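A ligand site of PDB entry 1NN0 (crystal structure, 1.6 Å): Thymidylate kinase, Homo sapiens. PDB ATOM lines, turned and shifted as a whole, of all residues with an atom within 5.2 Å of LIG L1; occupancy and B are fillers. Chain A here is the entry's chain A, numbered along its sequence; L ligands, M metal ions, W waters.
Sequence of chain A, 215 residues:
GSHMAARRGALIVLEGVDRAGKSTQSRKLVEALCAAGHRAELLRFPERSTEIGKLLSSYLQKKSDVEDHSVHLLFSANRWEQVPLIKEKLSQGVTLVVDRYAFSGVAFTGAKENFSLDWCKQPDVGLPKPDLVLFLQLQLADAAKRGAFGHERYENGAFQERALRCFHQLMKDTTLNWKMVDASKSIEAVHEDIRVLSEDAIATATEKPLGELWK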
ATOM      1  N   ASP A  18       3.340  17.690 -33.235  1.00  0.00           N
ATOM      2  CA  ASP A  18       2.739  18.648 -32.302  1.00  0.00           C
ATOM      3  C   ASP A  18       1.241  18.575 -32.268  1.00  0.00           C
ATOM      4  O   ASP A  18       0.581  18.478 -33.314  1.00  0.00           O
ATOM      5  CB  ASP A  18       3.224  20.061 -32.622  1.00  0.00           C
ATOM      6  CG  ASP A  18       3.047  21.005 -31.442  1.00  0.00           C
ATOM      7  OD1 ASP A  18       3.488  20.670 -30.323  1.00  0.00           O
ATOM      8  OD2 ASP A  18       2.449  22.079 -31.675  1.00  0.00           O
ATOM      9  N   LYS A  22       0.231  13.175 -27.691  1.00  0.00           N
ATOM     10  CA  LYS A  22       1.117  12.405 -26.797  1.00  0.00           C
ATOM     11  C   LYS A  22       0.618  12.433 -25.352  1.00  0.00           C
ATOM     12  O   LYS A  22       0.794  11.415 -24.665  1.00  0.00           O
ATOM     13  CB  LYS A  22       2.577  12.843 -26.891  1.00  0.00           C
ATOM     14  CG  LYS A  22       3.146  12.780 -28.301  1.00  0.00           C
ATOM     15  CD  LYS A  22       4.476  13.472 -28.481  1.00  0.00           C
ATOM     16  CE  LYS A  22       4.464  14.975 -28.168  1.00  0.00           C
ATOM     17  NZ  LYS A  22       3.785  15.676 -29.322  1.00  0.00           N
ATOM     18  N   PHE A  45       9.152  13.611 -20.367  1.00  0.00           N
ATOM     19  CA  PHE A  45      10.372  14.330 -20.537  1.00  0.00           C
ATOM     20  C   PHE A  45      10.074  15.568 -21.414  1.00  0.00           C
ATOM     21  O   PHE A  45       9.268  15.463 -22.323  1.00  0.00           O
ATOM     22  CB  PHE A  45      11.547  13.494 -21.094  1.00  0.00           C
ATOM     23  CG  PHE A  45      11.927  12.393 -20.119  1.00  0.00           C
ATOM     24  CD1 PHE A  45      11.498  11.078 -20.289  1.00  0.00           C
ATOM     25  CD2 PHE A  45      12.679  12.752 -19.033  1.00  0.00           C
ATOM     26  CE1 PHE A  45      11.858  10.130 -19.341  1.00  0.00           C
ATOM     27  CE2 PHE A  45      13.019  11.815 -18.045  1.00  0.00           C
ATOM     28  CZ  PHE A  45      12.623  10.489 -18.238  1.00  0.00           C
ATOM     29  N   PRO A  46      10.596  16.714 -21.022  1.00  0.00           N
ATOM     30  CA  PRO A  46      11.430  16.888 -19.851  1.00  0.00           C
ATOM     31  C   PRO A  46      10.584  16.728 -18.576  1.00  0.00           C
ATOM     32  O   PRO A  46       9.397  17.061 -18.459  1.00  0.00           O
ATOM     33  CB  PRO A  46      11.873  18.357 -19.886  1.00  0.00           C
ATOM     34  CG  PRO A  46      10.799  18.966 -20.756  1.00  0.00           C
ATOM     35  CD  PRO A  46      10.393  17.985 -21.780  1.00  0.00           C
ATOM     36  N   ARG A  48      10.120  18.451 -15.515  1.00  0.00           N
ATOM     37  CA  ARG A  48      10.450  19.822 -15.098  1.00  0.00           C
ATOM     38  C   ARG A  48      10.594  20.078 -13.640  1.00  0.00           C
ATOM     39  O   ARG A  48      10.960  21.244 -13.293  1.00  0.00           O
ATOM     40  CB  ARG A  48       9.357  20.743 -15.662  1.00  0.00           C
ATOM     41  CG  ARG A  48       9.356  20.738 -17.192  1.00  0.00           C
ATOM     42  CD  ARG A  48       8.204  21.613 -17.691  1.00  0.00           C
ATOM     43  NE  ARG A  48       7.906  21.314 -19.104  1.00  0.00           N
ATOM     44  CZ  ARG A  48       7.784  22.380 -19.910  1.00  0.00           C
ATOM     45  NH1 ARG A  48       7.954  23.590 -19.435  1.00  0.00           N
ATOM     46  NH2 ARG A  48       7.497  22.253 -21.184  1.00  0.00           N
ATOM     47  N   LEU A  60      12.326  26.640 -22.258  1.00  0.00           N
ATOM     48  CA  LEU A  60      11.176  26.392 -23.158  1.00  0.00           C
ATOM     49  C   LEU A  60      10.181  27.548 -23.061  1.00  0.00           C
ATOM     50  O   LEU A  60       9.486  27.810 -24.054  1.00  0.00           O
ATOM     51  CB  LEU A  60      10.512  25.048 -22.827  1.00  0.00           C
ATOM     52  CG  LEU A  60      11.353  23.825 -23.210  1.00  0.00           C
ATOM     53  CD1 LEU A  60      10.728  22.559 -22.621  1.00  0.00           C
ATOM     54  CD2 LEU A  60      11.594  23.692 -24.711  1.00  0.00           C
ATOM     55  N   PHE A  75      18.871  18.365 -21.474  1.00  0.00           N
ATOM     56  CA  PHE A  75      17.747  17.532 -21.828  1.00  0.00           C
ATOM     57  C   PHE A  75      18.109  16.024 -21.686  1.00  0.00           C
ATOM     58  O   PHE A  75      17.362  15.321 -21.066  1.00  0.00           O
ATOM     59  CB  PHE A  75      17.234  17.825 -23.243  1.00  0.00           C
ATOM     60  CG  PHE A  75      16.179  18.881 -23.418  1.00  0.00           C
ATOM     61  CD1 PHE A  75      16.445  19.986 -24.207  1.00  0.00           C
ATOM     62  CD2 PHE A  75      14.924  18.756 -22.779  1.00  0.00           C
ATOM     63  CE1 PHE A  75      15.469  20.961 -24.403  1.00  0.00           C
ATOM     64  CE2 PHE A  75      13.933  19.699 -22.997  1.00  0.00           C
ATOM     65  CZ  PHE A  75      14.244  20.810 -23.777  1.00  0.00           C
ATOM     66  N   ARG A  79      17.010  12.977 -18.480  1.00  0.00           N
ATOM     67  CA  ARG A  79      16.670  11.566 -18.645  1.00  0.00           C
ATOM     68  C   ARG A  79      17.560  10.711 -17.738  1.00  0.00           C
ATOM     69  O   ARG A  79      17.005   9.920 -16.988  1.00  0.00           O
ATOM     70  CB  ARG A  79      16.794  11.118 -20.096  1.00  0.00           C
ATOM     71  CG  ARG A  79      15.555  11.657 -20.825  1.00  0.00           C
ATOM     72  CD  ARG A  79      15.627  11.259 -22.256  1.00  0.00           C
ATOM     73  NE  ARG A  79      16.598  11.904 -23.097  1.00  0.00           N
ATOM     74  CZ  ARG A  79      16.457  13.156 -23.593  1.00  0.00           C
ATOM     75  NH1 ARG A  79      15.371  13.846 -23.304  1.00  0.00           N
ATOM     76  NH2 ARG A  79      17.372  13.634 -24.455  1.00  0.00           N
ATOM     77  N   ASP A  99       5.957  10.047 -21.896  1.00  0.00           N
ATOM     78  CA  ASP A  99       5.547  11.097 -22.864  1.00  0.00           C
ATOM     79  C   ASP A  99       6.829  11.833 -23.241  1.00  0.00           C
ATOM     80  O   ASP A  99       7.277  12.738 -22.456  1.00  0.00           O
ATOM     81  CB  ASP A  99       4.530  11.954 -22.176  1.00  0.00           C
ATOM     82  CG  ASP A  99       3.950  13.175 -22.908  1.00  0.00           C
ATOM     83  OD1 ASP A  99       4.346  13.446 -24.042  1.00  0.00           O
ATOM     84  OD2 ASP A  99       3.156  13.842 -22.188  1.00  0.00           O
ATOM     85  N   ARG A 100       7.298  11.527 -24.417  1.00  0.00           N
ATOM     86  CA  ARG A 100       8.552  11.954 -24.997  1.00  0.00           C
ATOM     87  C   ARG A 100       9.762  11.264 -24.316  1.00  0.00           C
ATOM     88  O   ARG A 100       9.783  11.058 -23.114  1.00  0.00           O
ATOM     89  CB  ARG A 100       8.838  13.471 -24.936  1.00  0.00           C
ATOM     90  CG  ARG A 100       7.769  14.198 -25.820  1.00  0.00           C
ATOM     91  CD  ARG A 100       8.249  15.670 -25.810  1.00  0.00           C
ATOM     92  NE  ARG A 100       7.355  16.601 -26.526  1.00  0.00           N
ATOM     93  CZ  ARG A 100       7.280  16.868 -27.805  1.00  0.00           C
ATOM     94  NH1 ARG A 100       8.025  16.291 -28.750  1.00  0.00           N
ATOM     95  NH2 ARG A 100       6.332  17.770 -28.164  1.00  0.00           N
ATOM     96  N   TYR A 101      10.762  11.082 -25.168  1.00  0.00           N
ATOM     97  CA  TYR A 101      12.013  10.492 -24.664  1.00  0.00           C
ATOM     98  C   TYR A 101      13.200  11.018 -25.476  1.00  0.00           C
ATOM     99  O   TYR A 101      13.198  12.170 -25.939  1.00  0.00           O
ATOM    100  CB  TYR A 101      11.962   8.989 -24.756  1.00  0.00           C
ATOM    101  CG  TYR A 101      12.903   8.100 -23.932  1.00  0.00           C
ATOM    102  CD1 TYR A 101      12.986   8.269 -22.571  1.00  0.00           C
ATOM    103  CD2 TYR A 101      13.602   7.071 -24.565  1.00  0.00           C
ATOM    104  CE1 TYR A 101      13.758   7.428 -21.775  1.00  0.00           C
ATOM    105  CE2 TYR A 101      14.402   6.224 -23.798  1.00  0.00           C
ATOM    106  CZ  TYR A 101      14.441   6.419 -22.440  1.00  0.00           C
ATOM    107  OH  TYR A 101      15.211   5.599 -21.613  1.00  0.00           O
ATOM    108  N   SER A 104      12.624  12.738 -29.073  1.00  0.00           N
ATOM    109  CA  SER A 104      12.362  14.194 -29.083  1.00  0.00           C
ATOM    110  C   SER A 104      13.649  14.973 -28.866  1.00  0.00           C
ATOM    111  O   SER A 104      13.857  16.052 -29.428  1.00  0.00           O
ATOM    112  CB  SER A 104      11.307  14.531 -28.032  1.00  0.00           C
ATOM    113  OG  SER A 104       9.987  14.368 -28.499  1.00  0.00           O
ATOM    114  N   GLY A 105      14.544  14.452 -28.002  1.00  0.00           N
ATOM    115  CA  GLY A 105      15.808  15.179 -27.755  1.00  0.00           C
ATOM    116  C   GLY A 105      16.673  15.304 -29.041  1.00  0.00           C
ATOM    117  O   GLY A 105      17.144  16.400 -29.297  1.00  0.00           O
ATOM    118  N   PHE A 108      14.574  17.571 -31.914  1.00  0.00           N
ATOM    119  CA  PHE A 108      14.471  18.990 -31.610  1.00  0.00           C
ATOM    120  C   PHE A 108      15.804  19.672 -31.740  1.00  0.00           C
ATOM    121  O   PHE A 108      15.900  20.740 -32.360  1.00  0.00           O
ATOM    122  CB  PHE A 108      13.674  19.194 -30.321  1.00  0.00           C
ATOM    123  CG  PHE A 108      12.212  19.114 -30.653  1.00  0.00           C
ATOM    124  CD1 PHE A 108      11.577  17.882 -30.751  1.00  0.00           C
ATOM    125  CD2 PHE A 108      11.470  20.274 -30.911  1.00  0.00           C
ATOM    126  CE1 PHE A 108      10.235  17.783 -31.066  1.00  0.00           C
ATOM    127  CE2 PHE A 108      10.108  20.160 -31.204  1.00  0.00           C
ATOM    128  CZ  PHE A 108       9.507  18.917 -31.324  1.00  0.00           C
ATOM    129  N   THR A 109      16.900  19.129 -31.216  1.00  0.00           N
ATOM    130  CA  THR A 109      18.191  19.733 -31.452  1.00  0.00           C
ATOM    131  C   THR A 109      18.647  19.511 -32.889  1.00  0.00           C
ATOM    132  O   THR A 109      19.189  20.418 -33.533  1.00  0.00           O
ATOM    133  CB  THR A 109      19.244  19.135 -30.466  1.00  0.00           C
ATOM    134  OG1 THR A 109      18.738  19.501 -29.171  1.00  0.00           O
ATOM    135  CG2 THR A 109      20.620  19.694 -30.808  1.00  0.00           C
ATOM    136  N   GLU A 152       5.565  28.523 -26.447  1.00  0.00           N
ATOM    137  CA  GLU A 152       6.857  28.014 -25.998  1.00  0.00           C
ATOM    138  C   GLU A 152       7.799  27.959 -27.206  1.00  0.00           C
ATOM    139  O   GLU A 152       7.447  27.969 -28.388  1.00  0.00           O
ATOM    140  CB  GLU A 152       6.794  26.639 -25.318  1.00  0.00           C
ATOM    141  CG  GLU A 152       6.255  26.630 -23.893  1.00  0.00           C
ATOM    142  CD  GLU A 152       6.663  25.519 -22.965  1.00  0.00           C
ATOM    143  OE1 GLU A 152       7.010  24.367 -23.344  1.00  0.00           O
ATOM    144  OE2 GLU A 152       6.629  25.752 -21.725  1.00  0.00           O
ATOM    145  N   TYR A 154      10.165  26.548 -30.057  1.00  0.00           N
ATOM    146  CA  TYR A 154       9.952  25.499 -31.027  1.00  0.00           C
ATOM    147  C   TYR A 154       8.518  25.421 -31.561  1.00  0.00           C
ATOM    148  O   TYR A 154       8.255  24.538 -32.388  1.00  0.00           O
ATOM    149  CB  TYR A 154      10.336  24.160 -30.385  1.00  0.00           C
ATOM    150  CG  TYR A 154      11.750  24.071 -29.843  1.00  0.00           C
ATOM    151  CD1 TYR A 154      11.963  23.288 -28.712  1.00  0.00           C
ATOM    152  CD2 TYR A 154      12.837  24.706 -30.402  1.00  0.00           C
ATOM    153  CE1 TYR A 154      13.239  23.129 -28.202  1.00  0.00           C
ATOM    154  CE2 TYR A 154      14.122  24.576 -29.911  1.00  0.00           C
ATOM    155  CZ  TYR A 154      14.317  23.784 -28.801  1.00  0.00           C
ATOM    156  OH  TYR A 154      15.542  23.584 -28.215  1.00  0.00           O
HETATM  157  P1  LIG L   1       5.785  19.282 -24.591  1.00  0.00           P
HETATM  158  O1  LIG L   1       6.095  17.834 -24.348  1.00  0.00           O
HETATM  159  O2  LIG L   1       4.907  19.913 -23.582  1.00  0.00           O
HETATM  160  O3  LIG L   1       5.360  19.367 -26.077  1.00  0.00           O
HETATM  161  O4  LIG L   1       7.027  20.221 -24.478  1.00  0.00           O
HETATM  162  N1  LIG L   1      12.169  18.670 -26.115  1.00  0.00           N
HETATM  163  C1  LIG L   1      11.766  17.619 -25.362  1.00  0.00           C
HETATM  164  C2  LIG L   1      13.487  18.925 -26.524  1.00  0.00           C
HETATM  165  O5  LIG L   1      13.854  19.859 -27.221  1.00  0.00           O
HETATM  166  N2  LIG L   1      14.379  17.963 -26.097  1.00  0.00           N
HETATM  167  C3  LIG L   1      14.065  16.889 -25.349  1.00  0.00           C
HETATM  168  O6  LIG L   1      14.951  16.010 -24.874  1.00  0.00           O
HETATM  169  C4  LIG L   1      12.706  16.724 -24.886  1.00  0.00           C
HETATM  170  C5  LIG L   1      12.418  15.495 -24.058  1.00  0.00           C
HETATM  171  C6  LIG L   1      10.200  19.269 -27.331  1.00  0.00           C
HETATM  172  C7  LIG L   1       8.362  19.920 -24.508  1.00  0.00           C
HETATM  173  C8  LIG L   1       9.242  20.662 -25.561  1.00  0.00           C
HETATM  174  O7  LIG L   1      10.582  20.209 -25.221  1.00  0.00           O
HETATM  175  C9  LIG L   1      11.221  19.735 -26.332  1.00  0.00           C
HETATM  176  C10 LIG L   1       8.994  20.105 -26.985  1.00  0.00           C
HETATM  177  P1  LG2 L   2       0.718  16.682 -27.484  1.00  0.00           P
HETATM  178  O1  LG2 L   2       1.056  15.718 -28.518  1.00  0.00           O
HETATM  179  O2  LG2 L   2       1.088  16.326 -26.091  1.00  0.00           O
HETATM  180  O3  LG2 L   2       1.065  18.200 -27.774  1.00  0.00           O
HETATM  181  P2  LG2 L   2      -2.072  16.835 -26.430  1.00  0.00           P
HETATM  182  O4  LG2 L   2      -1.694  17.938 -25.538  1.00  0.00           O
HETATM  183  O5  LG2 L   2      -2.285  15.431 -25.999  1.00  0.00           O
HETATM  184  O6  LG2 L   2      -0.932  16.786 -27.524  1.00  0.00           O
HETATM  185  O7  LG2 L   2      -3.281  17.283 -27.384  1.00  0.00           O
HETATM  186  C1  LG2 L   2      -3.290  18.572 -28.000  1.00  0.00           C
HETATM  187  C2  LG2 L   2      -4.716  19.112 -27.996  1.00  0.00           C
HETATM  188  O8  LG2 L   2      -5.478  18.307 -28.932  1.00  0.00           O
HETATM  189  C3  LG2 L   2      -5.442  19.039 -26.662  1.00  0.00           C
HETATM  190  O9  LG2 L   2      -6.369  20.097 -26.618  1.00  0.00           O
HETATM  191  C4  LG2 L   2      -6.190  17.697 -26.796  1.00  0.00           C
HETATM  192  O10 LG2 L   2      -7.367  17.595 -26.029  1.00  0.00           O
HETATM  193  C5  LG2 L   2      -6.529  17.674 -28.297  1.00  0.00           C
HETATM  194  N1  LG2 L   2      -6.555  16.274 -28.820  1.00  0.00           N
HETATM  195  C6  LG2 L   2      -5.656  15.280 -28.451  1.00  0.00           C
HETATM  196  N2  LG2 L   2      -5.926  14.162 -29.149  1.00  0.00           N
HETATM  197  C7  LG2 L   2      -6.972  14.491 -30.042  1.00  0.00           C
HETATM  198  C8  LG2 L   2      -7.629  13.760 -31.033  1.00  0.00           C
HETATM  199  N3  LG2 L   2      -7.400  12.516 -31.358  1.00  0.00           N
HETATM  200  N4  LG2 L   2      -8.600  14.444 -31.628  1.00  0.00           N
HETATM  201  C9  LG2 L   2      -8.913  15.724 -31.355  1.00  0.00           C
HETATM  202  N5  LG2 L   2      -8.330  16.474 -30.436  1.00  0.00           N
HETATM  203  C10 LG2 L   2      -7.365  15.772 -29.849  1.00  0.00           C
HETATM  204 MG    MG M   1       2.102  17.085 -24.570  1.00  0.00          MG
HETATM  205  O   HOH W   1      16.258  21.045 -27.911  1.00  0.00           O
HETATM  206  O   HOH W   2       3.958  15.978 -24.877  1.00  0.00           O
HETATM  207  O   HOH W   3       3.038  18.039 -22.905  1.00  0.00           O
HETATM  208  O   HOH W   4       6.502  19.988 -21.498  1.00  0.00           O
HETATM  209  O   HOH W   5       6.654  16.007 -22.248  1.00  0.00           O
HETATM  210  O   HOH W   6      17.107  18.039 -26.938  1.00  0.00           O
HETATM  211  O   HOH W   7       2.995  18.646 -25.879  1.00  0.00           O
HETATM  212  O   HOH W   8       8.017  23.556 -26.986  1.00  0.00           O
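Water W7 lies within hydrogen-bond range of O3 of LIG L1 and O3 of LG2 L2. Water W4 bridges NH2 of Arg 48 (2.5 Å) and O2 of LIG L1 (2.6 Å). Water W1 lies within hydrogen-bond range of the side-chain hydroxyl of Tyr 154 (2.7 Å), an oxygen (O5) of LIG L1 (2.8 Å) and the side-chain hydroxyl of Thr 109 (3.2 Å). Water W5 lies within hydrogen-bond range of O of Phe 45 (2.7 Å), O1 of LIG L1 (2.8 Å) and O of Asp 99 (3.3 Å). Water W6 lies within hydrogen-bond range of a nitrogen (N2) of LIG L1, the backbone carbonyl oxygen of Gly 105 and the side-chain hydroxyl of Thr 109. Water W2 lies within hydrogen-bond range of OD1 of Asp 99 (2.7 Å) and O1 of LIG L1 (2.9 Å).
NH1 of Arg 79 lies within hydrogen-bond range of O6 of LIG L1 (2.7 Å). The guanidinium group (NE) of Arg 100 lies within salt-bridge range of an oxygen (O1) of LIG L1. The backbone NH of Lys 22 sits at hydrogen-bond distance from an oxygen (O1) of LG2 L2, 2.8 Å away. An oxygen (O1) of LG2 L2 lies within salt-bridge range of the side-chain amino group (NZ) of Lys 22.
The backbone carbonyl oxygen (O) of Phe 75 sits at hydrogen-bond distance from the guanidinium group (NH1) of Arg 79, at 3.3 Å. NH1 of Arg 100 lies within hydrogen-bond range of OG of Ser 104. O of Gly 105 is in hydrogen-bond range of OG1 of Thr 109. N of Phe 45 lies within hydrogen-bond range of O of Asp 99, at 2.9 Å. The side-chain carboxylate (OE1) of Glu 152 is in salt-bridge range of the guanidinium group (NH2) of Arg 48 (3.1 Å).
C of Phe 45 touches C5 of LIG L1, 3.5 Å away. N of Pro 46 touches C5 of LIG L1 (3.7 Å). NH2 of Arg 48 touches O4 of LIG L1, 3.9 Å away. CD1 of Leu 60 touches O7 of LIG L1, 3.5 Å away. Phe 75 touches LIG L1. Tyr 101 touches LIG L1 (O to C5, 3.9 Å). Ser 104 touches LIG L1. Gly 105 touches LIG L1. Phe 108 touches LIG L1. Tyr 154 touches LIG L1. Hydrophobic or aromatic side chains within 4 Å of LIG L1: Phe 45, Pro 46, Leu 60, Phe 75, Phe 108 and Tyr 154. 12 residues have an atom within 4 Å of LIG L1: Phe 45, Pro 46, Arg 48, Leu 60, Phe 75, Arg 79, Arg 100, Tyr 101, Ser 104, Gly 105, Phe 108 and Tyr 154. Along chain A the residues within 4 Å of LIG L1 span positions 45 to 154. The nearest printed residue that does not touch LIG L1 is Glu 152 (4.3 Å).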
